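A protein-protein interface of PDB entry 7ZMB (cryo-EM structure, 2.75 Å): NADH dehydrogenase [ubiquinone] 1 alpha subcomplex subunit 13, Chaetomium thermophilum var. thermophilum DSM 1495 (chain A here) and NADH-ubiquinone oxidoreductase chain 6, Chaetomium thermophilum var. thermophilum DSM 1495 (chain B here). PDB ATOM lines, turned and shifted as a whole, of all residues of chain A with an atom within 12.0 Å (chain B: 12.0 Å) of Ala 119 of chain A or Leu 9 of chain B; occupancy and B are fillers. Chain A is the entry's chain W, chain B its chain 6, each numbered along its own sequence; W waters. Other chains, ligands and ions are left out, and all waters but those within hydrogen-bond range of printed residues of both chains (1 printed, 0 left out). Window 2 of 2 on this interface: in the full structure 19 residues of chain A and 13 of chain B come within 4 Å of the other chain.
Of the 12 printed residues of chain A, 8 touch a printed residue of chain B.
Printed residues of chain A that touch a printed residue of chain B: Arg 89, Ala 112, Val 113, Thr 114, Pro 115, Lys 117, Pro 118 and Ala 119.
Hydrophobic or aromatic side chains of chain A within 4 Å of the printed part of chain B: Ala 112, Pro 115, Pro 118 and Ala 119.
Printed residues of chain B that touch a printed residue of chain A: Ser 6, Leu 7, Leu 9, Phe 168 and Ile 170.
Hydrophobic or aromatic side chains of chain B within 4 Å of the printed part of chain A: Leu 7, Leu 9, Phe 168 and Ile 170.
Among the printed residues, no Asp or Glu carboxylate lies within 4 Å of a Lys or Arg side-chain nitrogen of the other chain.
The backbone NH of Ala 112 of chain A is in hydrogen-bond range of the backbone carbonyl oxygen of Phe 168 of chain B (3.3 Å).
The guanidinium group (NH1) of Arg 89 of chain A is in hydrogen-bond range of the backbone carbonyl oxygen (O) of Ser 6 of chain B (3.1 Å).
The backbone NH (N) of Ala 119 of chain A lies within hydrogen-bond range of the backbone carbonyl oxygen (O) of Leu 9 of chain B (2.7 Å).
Of the printed residues of chain B, Val 113 of chain A touches Leu 7 (3.5 Å).
Of chain B, only Phe 168 comes within 4 Å of Thr 114 of chain A.
Pro 115 of chain A touches just these residues of chain B: Leu 7 and Leu 9.
Of chain B, only Leu 9 (3.4 Å) comes within 4 Å of Pro 118 of chain A.
Ala 119 of chain A touches one residue of chain B.
No residue of chain B comes within 4 Å of Gln 120 of chain A.
No residue of chain B comes within 4 Å of Glu 121 of chain A.
Ile 5 of chain B touches none of the printed residues of chain A.
Leu 7 of chain B touches just these residues of chain A: Arg 89 (3.7 Å), Val 113 (3.5 Å) and Pro 115 (3.9 Å).
No residue of chain A comes within 4 Å of Leu 8 of chain B.
Leu 9 of chain B touches just these residues of chain A: Pro 115, Lys 117, Pro 118 and Ala 119.
No residue of chain A comes within 4 Å of Leu 10 of chain B.
Leu 167 of chain B touches none of the printed residues of chain A.
Of the printed residues of chain A, Phe 168 of chain B touches Ala 112 and Thr 114.
The nearest residue of chain A that does not touch Leu 9 of chain B is Thr 114 of chain A (4.1 Å).
The nearest printed residue of chain B that does not touch Ala 112 of chain A is Phe 169 of chain B (5.2 Å).
Water W1 bridges O of Ala 112 of chain A (2.8 Å) and N of Phe 168 of chain B (3.1 Å).
Among the printed residues, merely in contact across the chains: Arg 89 of chain A with Leu 7 of chain B, Ala 112 of chain A with Ile 170 of chain B, Val 113 of chain A with Leu 7 of chain B, Thr 114 of chain A with Phe 168 of chain B, Pro 115 of chain A with Leu 7 of chain B, Pro 115 of chain A with Leu 9 of chain B, Lys 117 of chain A with Leu 9 of chain B and Pro 118 of chain A with Leu 9 of chain B.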
ATOM      1  N   ARG A  82       7.555  18.225  -5.885  1.00  0.00           N
ATOM      2  CA  ARG A  82       6.166  17.909  -5.468  1.00  0.00           C
ATOM      3  C   ARG A  82       5.837  16.444  -5.694  1.00  0.00           C
ATOM      4  O   ARG A  82       4.977  15.938  -4.975  1.00  0.00           O
ATOM      5  CB  ARG A  82       5.167  18.873  -6.119  1.00  0.00           C
ATOM      6  CG  ARG A  82       5.444  20.336  -5.804  1.00  0.00           C
ATOM      7  CD  ARG A  82       4.451  21.348  -6.334  1.00  0.00           C
ATOM      8  NE  ARG A  82       3.116  21.158  -5.795  1.00  0.00           N
ATOM      9  CZ  ARG A  82       2.174  22.091  -5.763  1.00  0.00           C
ATOM     10  NH1 ARG A  82       0.987  21.811  -5.255  1.00  0.00           N
ATOM     11  NH2 ARG A  82       2.424  23.300  -6.226  1.00  0.00           N
ATOM     12  N   ARG A  89       3.582  11.560   0.981  1.00  0.00           N
ATOM     13  CA  ARG A  89       2.270  11.811   1.558  1.00  0.00           C
ATOM     14  C   ARG A  89       1.306  10.645   1.357  1.00  0.00           C
ATOM     15  O   ARG A  89       0.317  10.541   2.086  1.00  0.00           O
ATOM     16  CB  ARG A  89       1.696  13.104   0.964  1.00  0.00           C
ATOM     17  CG  ARG A  89       0.486  13.663   1.692  1.00  0.00           C
ATOM     18  CD  ARG A  89      -0.095  14.874   0.975  1.00  0.00           C
ATOM     19  NE  ARG A  89       0.936  15.801   0.513  1.00  0.00           N
ATOM     20  CZ  ARG A  89       1.281  16.914   1.149  1.00  0.00           C
ATOM     21  NH1 ARG A  89       2.230  17.695   0.654  1.00  0.00           N
ATOM     22  NH2 ARG A  89       0.678  17.250   2.277  1.00  0.00           N
ATOM     23  N   ALA A 112      -4.875  16.575  -8.492  1.00  0.00           N
ATOM     24  CA  ALA A 112      -4.104  16.794  -7.283  1.00  0.00           C
ATOM     25  C   ALA A 112      -5.023  16.706  -6.080  1.00  0.00           C
ATOM     26  O   ALA A 112      -6.193  17.084  -6.144  1.00  0.00           O
ATOM     27  CB  ALA A 112      -3.398  18.150  -7.288  1.00  0.00           C
ATOM     28  N   VAL A 113      -4.479  16.188  -4.982  1.00  0.00           N
ATOM     29  CA  VAL A 113      -5.172  16.248  -3.706  1.00  0.00           C
ATOM     30  C   VAL A 113      -5.100  17.667  -3.162  1.00  0.00           C
ATOM     31  O   VAL A 113      -4.023  18.274  -3.104  1.00  0.00           O
ATOM     32  CB  VAL A 113      -4.570  15.240  -2.722  1.00  0.00           C
ATOM     33  CG1 VAL A 113      -5.217  15.384  -1.373  1.00  0.00           C
ATOM     34  CG2 VAL A 113      -4.768  13.846  -3.246  1.00  0.00           C
ATOM     35  N   THR A 114      -6.245  18.207  -2.780  1.00  0.00           N
ATOM     36  CA  THR A 114      -6.347  19.527  -2.190  1.00  0.00           C
ATOM     37  C   THR A 114      -6.893  19.420  -0.776  1.00  0.00           C
ATOM     38  O   THR A 114      -7.579  18.450  -0.436  1.00  0.00           O
ATOM     39  CB  THR A 114      -7.266  20.442  -3.017  1.00  0.00           C
ATOM     40  OG1 THR A 114      -8.635  20.144  -2.722  1.00  0.00           O
ATOM     41  CG2 THR A 114      -7.026  20.260  -4.499  1.00  0.00           C
ATOM     42  N   PRO A 115      -6.604  20.396   0.082  1.00  0.00           N
ATOM     43  CA  PRO A 115      -7.305  20.473   1.363  1.00  0.00           C
ATOM     44  C   PRO A 115      -8.769  20.820   1.163  1.00  0.00           C
ATOM     45  O   PRO A 115      -9.178  21.349   0.128  1.00  0.00           O
ATOM     46  CB  PRO A 115      -6.561  21.584   2.108  1.00  0.00           C
ATOM     47  CG  PRO A 115      -5.945  22.394   1.042  1.00  0.00           C
ATOM     48  CD  PRO A 115      -5.570  21.436  -0.034  1.00  0.00           C
ATOM     49  N   SER A 116      -9.568  20.503   2.178  1.00  0.00           N
ATOM     50  CA  SER A 116     -11.008  20.685   2.083  1.00  0.00           C
ATOM     51  C   SER A 116     -11.435  22.143   2.139  1.00  0.00           C
ATOM     52  O   SER A 116     -12.593  22.439   1.827  1.00  0.00           O
ATOM     53  CB  SER A 116     -11.708  19.908   3.197  1.00  0.00           C
ATOM     54  OG  SER A 116     -13.093  20.202   3.223  1.00  0.00           O
ATOM     55  N   LYS A 117     -10.549  23.054   2.522  1.00  0.00           N
ATOM     56  CA  LYS A 117     -10.887  24.461   2.651  1.00  0.00           C
ATOM     57  C   LYS A 117      -9.753  25.312   2.100  1.00  0.00           C
ATOM     58  O   LYS A 117      -8.583  24.924   2.191  1.00  0.00           O
ATOM     59  CB  LYS A 117     -11.157  24.830   4.121  1.00  0.00           C
ATOM     60  CG  LYS A 117     -11.804  26.191   4.340  1.00  0.00           C
ATOM     61  CD  LYS A 117     -12.105  26.444   5.809  1.00  0.00           C
ATOM     62  CE  LYS A 117     -13.460  25.877   6.205  1.00  0.00           C
ATOM     63  NZ  LYS A 117     -13.956  26.462   7.480  1.00  0.00           N
ATOM     64  N   PRO A 118     -10.034  26.464   1.429  1.00  0.00           N
ATOM     65  CA  PRO A 118      -8.985  27.409   1.010  1.00  0.00           C
ATOM     66  C   PRO A 118      -8.564  28.311   2.185  1.00  0.00           C
ATOM     67  O   PRO A 118      -9.262  28.317   3.190  1.00  0.00           O
ATOM     68  CB  PRO A 118      -9.619  28.267  -0.096  1.00  0.00           C
ATOM     69  CG  PRO A 118     -10.926  27.589  -0.418  1.00  0.00           C
ATOM     70  CD  PRO A 118     -11.330  26.919   0.877  1.00  0.00           C
ATOM     71  N   ALA A 119      -7.465  29.052   2.043  1.00  0.00           N
ATOM     72  CA  ALA A 119      -6.960  29.858   3.179  1.00  0.00           C
ATOM     73  C   ALA A 119      -8.065  30.803   3.665  1.00  0.00           C
ATOM     74  O   ALA A 119      -8.747  31.405   2.814  1.00  0.00           O
ATOM     75  CB  ALA A 119      -5.718  30.612   2.776  1.00  0.00           C
ATOM     76  N   GLN A 120      -8.222  30.933   4.983  1.00  0.00           N
ATOM     77  CA  GLN A 120      -9.344  31.727   5.561  1.00  0.00           C
ATOM     78  C   GLN A 120      -9.457  33.131   4.956  1.00  0.00           C
ATOM     79  O   GLN A 120     -10.607  33.592   4.813  1.00  0.00           O
ATOM     80  CB  GLN A 120      -9.208  31.784   7.083  1.00  0.00           C
ATOM     81  CG  GLN A 120     -10.479  32.241   7.784  1.00  0.00           C
ATOM     82  CD  GLN A 120     -11.667  31.379   7.429  1.00  0.00           C
ATOM     83  OE1 GLN A 120     -11.598  30.152   7.450  1.00  0.00           O
ATOM     84  NE2 GLN A 120     -12.778  32.022   7.107  1.00  0.00           N
ATOM     85  N   GLU A 121      -8.330  33.787   4.645  1.00  0.00           N
ATOM     86  CA  GLU A 121      -8.358  35.152   4.125  1.00  0.00           C
ATOM     87  C   GLU A 121      -8.951  36.130   5.134  1.00  0.00           C
ATOM     88  O   GLU A 121      -8.861  35.919   6.343  1.00  0.00           O
ATOM     89  CB  GLU A 121      -9.142  35.214   2.810  1.00  0.00           C
ATOM     90  N   GLN B   4       2.547  20.492  10.688  1.00  0.00           N
ATOM     91  CA  GLN B   4       2.955  20.803   9.325  1.00  0.00           C
ATOM     92  C   GLN B   4       1.716  21.038   8.474  1.00  0.00           C
ATOM     93  O   GLN B   4       0.792  20.219   8.477  1.00  0.00           O
ATOM     94  CB  GLN B   4       3.803  19.672   8.733  1.00  0.00           C
ATOM     95  N   ILE B   5       1.699  22.158   7.749  1.00  0.00           N
ATOM     96  CA  ILE B   5       0.555  22.463   6.894  1.00  0.00           C
ATOM     97  C   ILE B   5       0.627  21.643   5.614  1.00  0.00           C
ATOM     98  O   ILE B   5      -0.244  20.808   5.338  1.00  0.00           O
ATOM     99  CB  ILE B   5       0.503  23.968   6.592  1.00  0.00           C
ATOM    100  CG1 ILE B   5       0.708  24.776   7.875  1.00  0.00           C
ATOM    101  CG2 ILE B   5      -0.833  24.318   5.983  1.00  0.00           C
ATOM    102  CD1 ILE B   5      -0.350  24.538   8.923  1.00  0.00           C
ATOM    103  N   SER B   6       1.656  21.896   4.806  1.00  0.00           N
ATOM    104  CA  SER B   6       2.113  21.035   3.710  1.00  0.00           C
ATOM    105  C   SER B   6       1.200  21.160   2.494  1.00  0.00           C
ATOM    106  O   SER B   6       1.579  20.656   1.424  1.00  0.00           O
ATOM    107  CB  SER B   6       2.289  19.619   4.263  1.00  0.00           C
ATOM    108  OG  SER B   6       3.149  19.614   5.390  1.00  0.00           O
ATOM    109  N   LEU B   7       0.008  21.754   2.608  1.00  0.00           N
ATOM    110  CA  LEU B   7      -0.804  21.942   1.368  1.00  0.00           C
ATOM    111  C   LEU B   7      -1.601  23.230   1.482  1.00  0.00           C
ATOM    112  O   LEU B   7      -2.401  23.335   2.426  1.00  0.00           O
ATOM    113  CB  LEU B   7      -1.725  20.751   1.069  1.00  0.00           C
ATOM    114  CG  LEU B   7      -1.151  19.630   0.195  1.00  0.00           C
ATOM    115  CD1 LEU B   7      -2.230  18.609  -0.134  1.00  0.00           C
ATOM    116  CD2 LEU B   7      -0.547  20.175  -1.086  1.00  0.00           C
ATOM    117  N   LEU B   8      -1.401  24.149   0.537  1.00  0.00           N
ATOM    118  CA  LEU B   8      -2.045  25.474   0.659  1.00  0.00           C
ATOM    119  C   LEU B   8      -3.066  25.676  -0.447  1.00  0.00           C
ATOM    120  O   LEU B   8      -2.666  25.687  -1.623  1.00  0.00           O
ATOM    121  CB  LEU B   8      -0.944  26.531   0.585  1.00  0.00           C
ATOM    122  CG  LEU B   8       0.093  26.429   1.703  1.00  0.00           C
ATOM    123  CD1 LEU B   8       1.162  27.495   1.564  1.00  0.00           C
ATOM    124  CD2 LEU B   8      -0.575  26.510   3.063  1.00  0.00           C
ATOM    125  N   LEU B   9      -4.330  25.858  -0.065  1.00  0.00           N
ATOM    126  CA  LEU B   9      -5.348  26.187  -1.080  1.00  0.00           C
ATOM    127  C   LEU B   9      -5.524  27.697  -0.974  1.00  0.00           C
ATOM    128  O   LEU B   9      -5.828  28.186   0.103  1.00  0.00           O
ATOM    129  CB  LEU B   9      -6.634  25.404  -0.806  1.00  0.00           C
ATOM    130  CG  LEU B   9      -7.454  25.001  -2.029  1.00  0.00           C
ATOM    131  CD1 LEU B   9      -8.589  24.075  -1.626  1.00  0.00           C
ATOM    132  CD2 LEU B   9      -8.006  26.220  -2.751  1.00  0.00           C
ATOM    133  N   LEU B  10      -5.282  28.402  -2.066  1.00  0.00           N
ATOM    134  CA  LEU B  10      -5.340  29.875  -2.046  1.00  0.00           C
ATOM    135  C   LEU B  10      -6.268  30.284  -3.176  1.00  0.00           C
ATOM    136  O   LEU B  10      -6.196  29.644  -4.223  1.00  0.00           O
ATOM    137  CB  LEU B  10      -3.915  30.339  -2.365  1.00  0.00           C
ATOM    138  CG  LEU B  10      -3.671  31.835  -2.280  1.00  0.00           C
ATOM    139  CD1 LEU B  10      -3.912  32.306  -0.858  1.00  0.00           C
ATOM    140  CD2 LEU B  10      -2.253  32.159  -2.722  1.00  0.00           C
ATOM    141  N   LYS B  11      -7.107  31.293  -2.966  1.00  0.00           N
ATOM    142  CA  LYS B  11      -7.926  31.821  -4.091  1.00  0.00           C
ATOM    143  C   LYS B  11      -7.020  32.628  -5.019  1.00  0.00           C
ATOM    144  O   LYS B  11      -6.200  33.407  -4.500  1.00  0.00           O
ATOM    145  CB  LYS B  11      -9.046  32.722  -3.568  1.00  0.00           C
ATOM    146  CG  LYS B  11      -9.957  33.321  -4.632  1.00  0.00           C
ATOM    147  CD  LYS B  11     -11.083  34.160  -4.071  1.00  0.00           C
ATOM    148  CE  LYS B  11     -12.018  33.367  -3.186  1.00  0.00           C
ATOM    149  NZ  LYS B  11     -13.133  34.202  -2.683  1.00  0.00           N
ATOM    150  N   GLU B  12      -7.192  32.472  -6.332  1.00  0.00           N
ATOM    151  CA  GLU B  12      -6.401  33.242  -7.325  1.00  0.00           C
ATOM    152  C   GLU B  12      -6.928  34.681  -7.400  1.00  0.00           C
ATOM    153  O   GLU B  12      -8.120  34.853  -7.679  1.00  0.00           O
ATOM    154  CB  GLU B  12      -6.530  32.547  -8.674  1.00  0.00           C
ATOM    155  CG  GLU B  12      -5.333  32.747  -9.580  1.00  0.00           C
ATOM    156  CD  GLU B  12      -5.351  31.830 -10.789  1.00  0.00           C
ATOM    157  OE1 GLU B  12      -6.114  30.848 -10.765  1.00  0.00           O
ATOM    158  OE2 GLU B  12      -4.618  32.107 -11.749  1.00  0.00           O
ATOM    159  N   ILE B  13      -6.059  35.665  -7.174  1.00  0.00           N
ATOM    160  CA  ILE B  13      -6.478  37.095  -7.139  1.00  0.00           C
ATOM    161  C   ILE B  13      -6.820  37.531  -8.563  1.00  0.00           C
ATOM    162  O   ILE B  13      -8.006  37.817  -8.817  1.00  0.00           O
ATOM    163  CB  ILE B  13      -5.439  37.967  -6.397  1.00  0.00           C
ATOM    164  CG1 ILE B  13      -5.921  39.408  -6.212  1.00  0.00           C
ATOM    165  CG2 ILE B  13      -4.041  37.874  -6.988  1.00  0.00           C
ATOM    166  CD1 ILE B  13      -5.052  40.237  -5.292  1.00  0.00           C
ATOM    167  N   ASN B  16      -7.139  34.558 -12.877  1.00  0.00           N
ATOM    168  CA  ASN B  16      -8.046  33.448 -12.675  1.00  0.00           C
ATOM    169  C   ASN B  16      -8.991  33.320 -13.866  1.00  0.00           C
ATOM    170  O   ASN B  16      -9.252  34.277 -14.596  1.00  0.00           O
ATOM    171  CB  ASN B  16      -8.838  33.635 -11.385  1.00  0.00           C
ATOM    172  CG  ASN B  16      -9.565  34.948 -11.339  1.00  0.00           C
ATOM    173  OD1 ASN B  16      -8.972  35.994 -11.092  1.00  0.00           O
ATOM    174  ND2 ASN B  16     -10.869  34.903 -11.563  1.00  0.00           N
ATOM    175  N   LYS B 164     -19.291  14.370  -1.578  1.00  0.00           N
ATOM    176  CA  LYS B 164     -18.725  15.636  -1.131  1.00  0.00           C
ATOM    177  C   LYS B 164     -17.206  15.640  -1.271  1.00  0.00           C
ATOM    178  O   LYS B 164     -16.527  16.518  -0.741  1.00  0.00           O
ATOM    179  CB  LYS B 164     -19.120  15.917   0.320  1.00  0.00           C
ATOM    180  N   ASN B 165     -16.680  14.650  -1.986  1.00  0.00           N
ATOM    181  CA  ASN B 165     -15.248  14.524  -2.241  1.00  0.00           C
ATOM    182  C   ASN B 165     -15.034  14.628  -3.748  1.00  0.00           C
ATOM    183  O   ASN B 165     -15.005  13.615  -4.451  1.00  0.00           O
ATOM    184  CB  ASN B 165     -14.687  13.213  -1.687  1.00  0.00           C
ATOM    185  N   ASP B 166     -14.886  15.852  -4.237  1.00  0.00           N
ATOM    186  CA  ASP B 166     -14.691  16.108  -5.655  1.00  0.00           C
ATOM    187  C   ASP B 166     -13.209  16.105  -6.000  1.00  0.00           C
ATOM    188  O   ASP B 166     -12.344  16.240  -5.136  1.00  0.00           O
ATOM    189  CB  ASP B 166     -15.318  17.446  -6.059  1.00  0.00           C
ATOM    190  CG  ASP B 166     -16.823  17.457  -5.901  1.00  0.00           C
ATOM    191  OD1 ASP B 166     -17.420  16.365  -5.799  1.00  0.00           O
ATOM    192  OD2 ASP B 166     -17.411  18.557  -5.883  1.00  0.00           O
ATOM    193  N   LEU B 167     -12.925  15.937  -7.284  1.00  0.00           N
ATOM    194  CA  LEU B 167     -11.563  16.020  -7.779  1.00  0.00           C
ATOM    195  C   LEU B 167     -11.306  17.410  -8.319  1.00  0.00           C
ATOM    196  O   LEU B 167     -12.231  18.140  -8.674  1.00  0.00           O
ATOM    197  CB  LEU B 167     -11.292  14.982  -8.867  1.00  0.00           C
ATOM    198  CG  LEU B 167     -11.180  13.554  -8.355  1.00  0.00           C
ATOM    199  CD1 LEU B 167     -10.693  12.630  -9.443  1.00  0.00           C
ATOM    200  CD2 LEU B 167     -10.274  13.497  -7.145  1.00  0.00           C
ATOM    201  N   PHE B 168     -10.031  17.774  -8.347  1.00  0.00           N
ATOM    202  CA  PHE B 168      -9.645  19.098  -8.886  1.00  0.00           C
ATOM    203  C   PHE B 168      -8.527  18.876  -9.898  1.00  0.00           C
ATOM    204  O   PHE B 168      -7.523  18.219  -9.566  1.00  0.00           O
ATOM    205  CB  PHE B 168      -9.275  20.062  -7.760  1.00  0.00           C
ATOM    206  CG  PHE B 168     -10.423  20.441  -6.858  1.00  0.00           C
ATOM    207  CD1 PHE B 168     -11.290  21.465  -7.204  1.00  0.00           C
ATOM    208  CD2 PHE B 168     -10.641  19.772  -5.665  1.00  0.00           C
ATOM    209  CE1 PHE B 168     -12.347  21.812  -6.378  1.00  0.00           C
ATOM    210  CE2 PHE B 168     -11.698  20.119  -4.839  1.00  0.00           C
ATOM    211  CZ  PHE B 168     -12.547  21.139  -5.197  1.00  0.00           C
ATOM    212  N   PHE B 169      -8.742  19.357 -11.121  1.00  0.00           N
ATOM    213  CA  PHE B 169      -7.687  19.257 -12.153  1.00  0.00           C
ATOM    214  C   PHE B 169      -6.570  20.224 -11.774  1.00  0.00           C
ATOM    215  O   PHE B 169      -6.867  21.342 -11.339  1.00  0.00           O
ATOM    216  CB  PHE B 169      -8.275  19.505 -13.543  1.00  0.00           C
ATOM    217  CG  PHE B 169      -9.364  18.561 -13.980  1.00  0.00           C
ATOM    218  CD1 PHE B 169      -9.058  17.374 -14.621  1.00  0.00           C
ATOM    219  CD2 PHE B 169     -10.697  18.871 -13.772  1.00  0.00           C
ATOM    220  CE1 PHE B 169     -10.061  16.514 -15.041  1.00  0.00           C
ATOM    221  CE2 PHE B 169     -11.698  18.006 -14.183  1.00  0.00           C
ATOM    222  CZ  PHE B 169     -11.378  16.829 -14.814  1.00  0.00           C
ATOM    223  N   ILE B 170      -5.322  19.783 -11.913  1.00  0.00           N
ATOM    224  CA  ILE B 170      -4.158  20.636 -11.550  1.00  0.00           C
ATOM    225  C   ILE B 170      -3.362  20.944 -12.820  1.00  0.00           C
ATOM    226  O   ILE B 170      -3.122  20.021 -13.609  1.00  0.00           O
ATOM    227  CB  ILE B 170      -3.323  19.977 -10.436  1.00  0.00           C
ATOM    228  CG1 ILE B 170      -2.300  20.941  -9.834  1.00  0.00           C
ATOM    229  CG2 ILE B 170      -2.700  18.662 -10.873  1.00  0.00           C
ATOM    230  CD1 ILE B 170      -2.893  21.896  -8.835  1.00  0.00           C
HETATM  231  O   HOH W   1      -8.876  17.114  -5.525  1.00  0.00           O
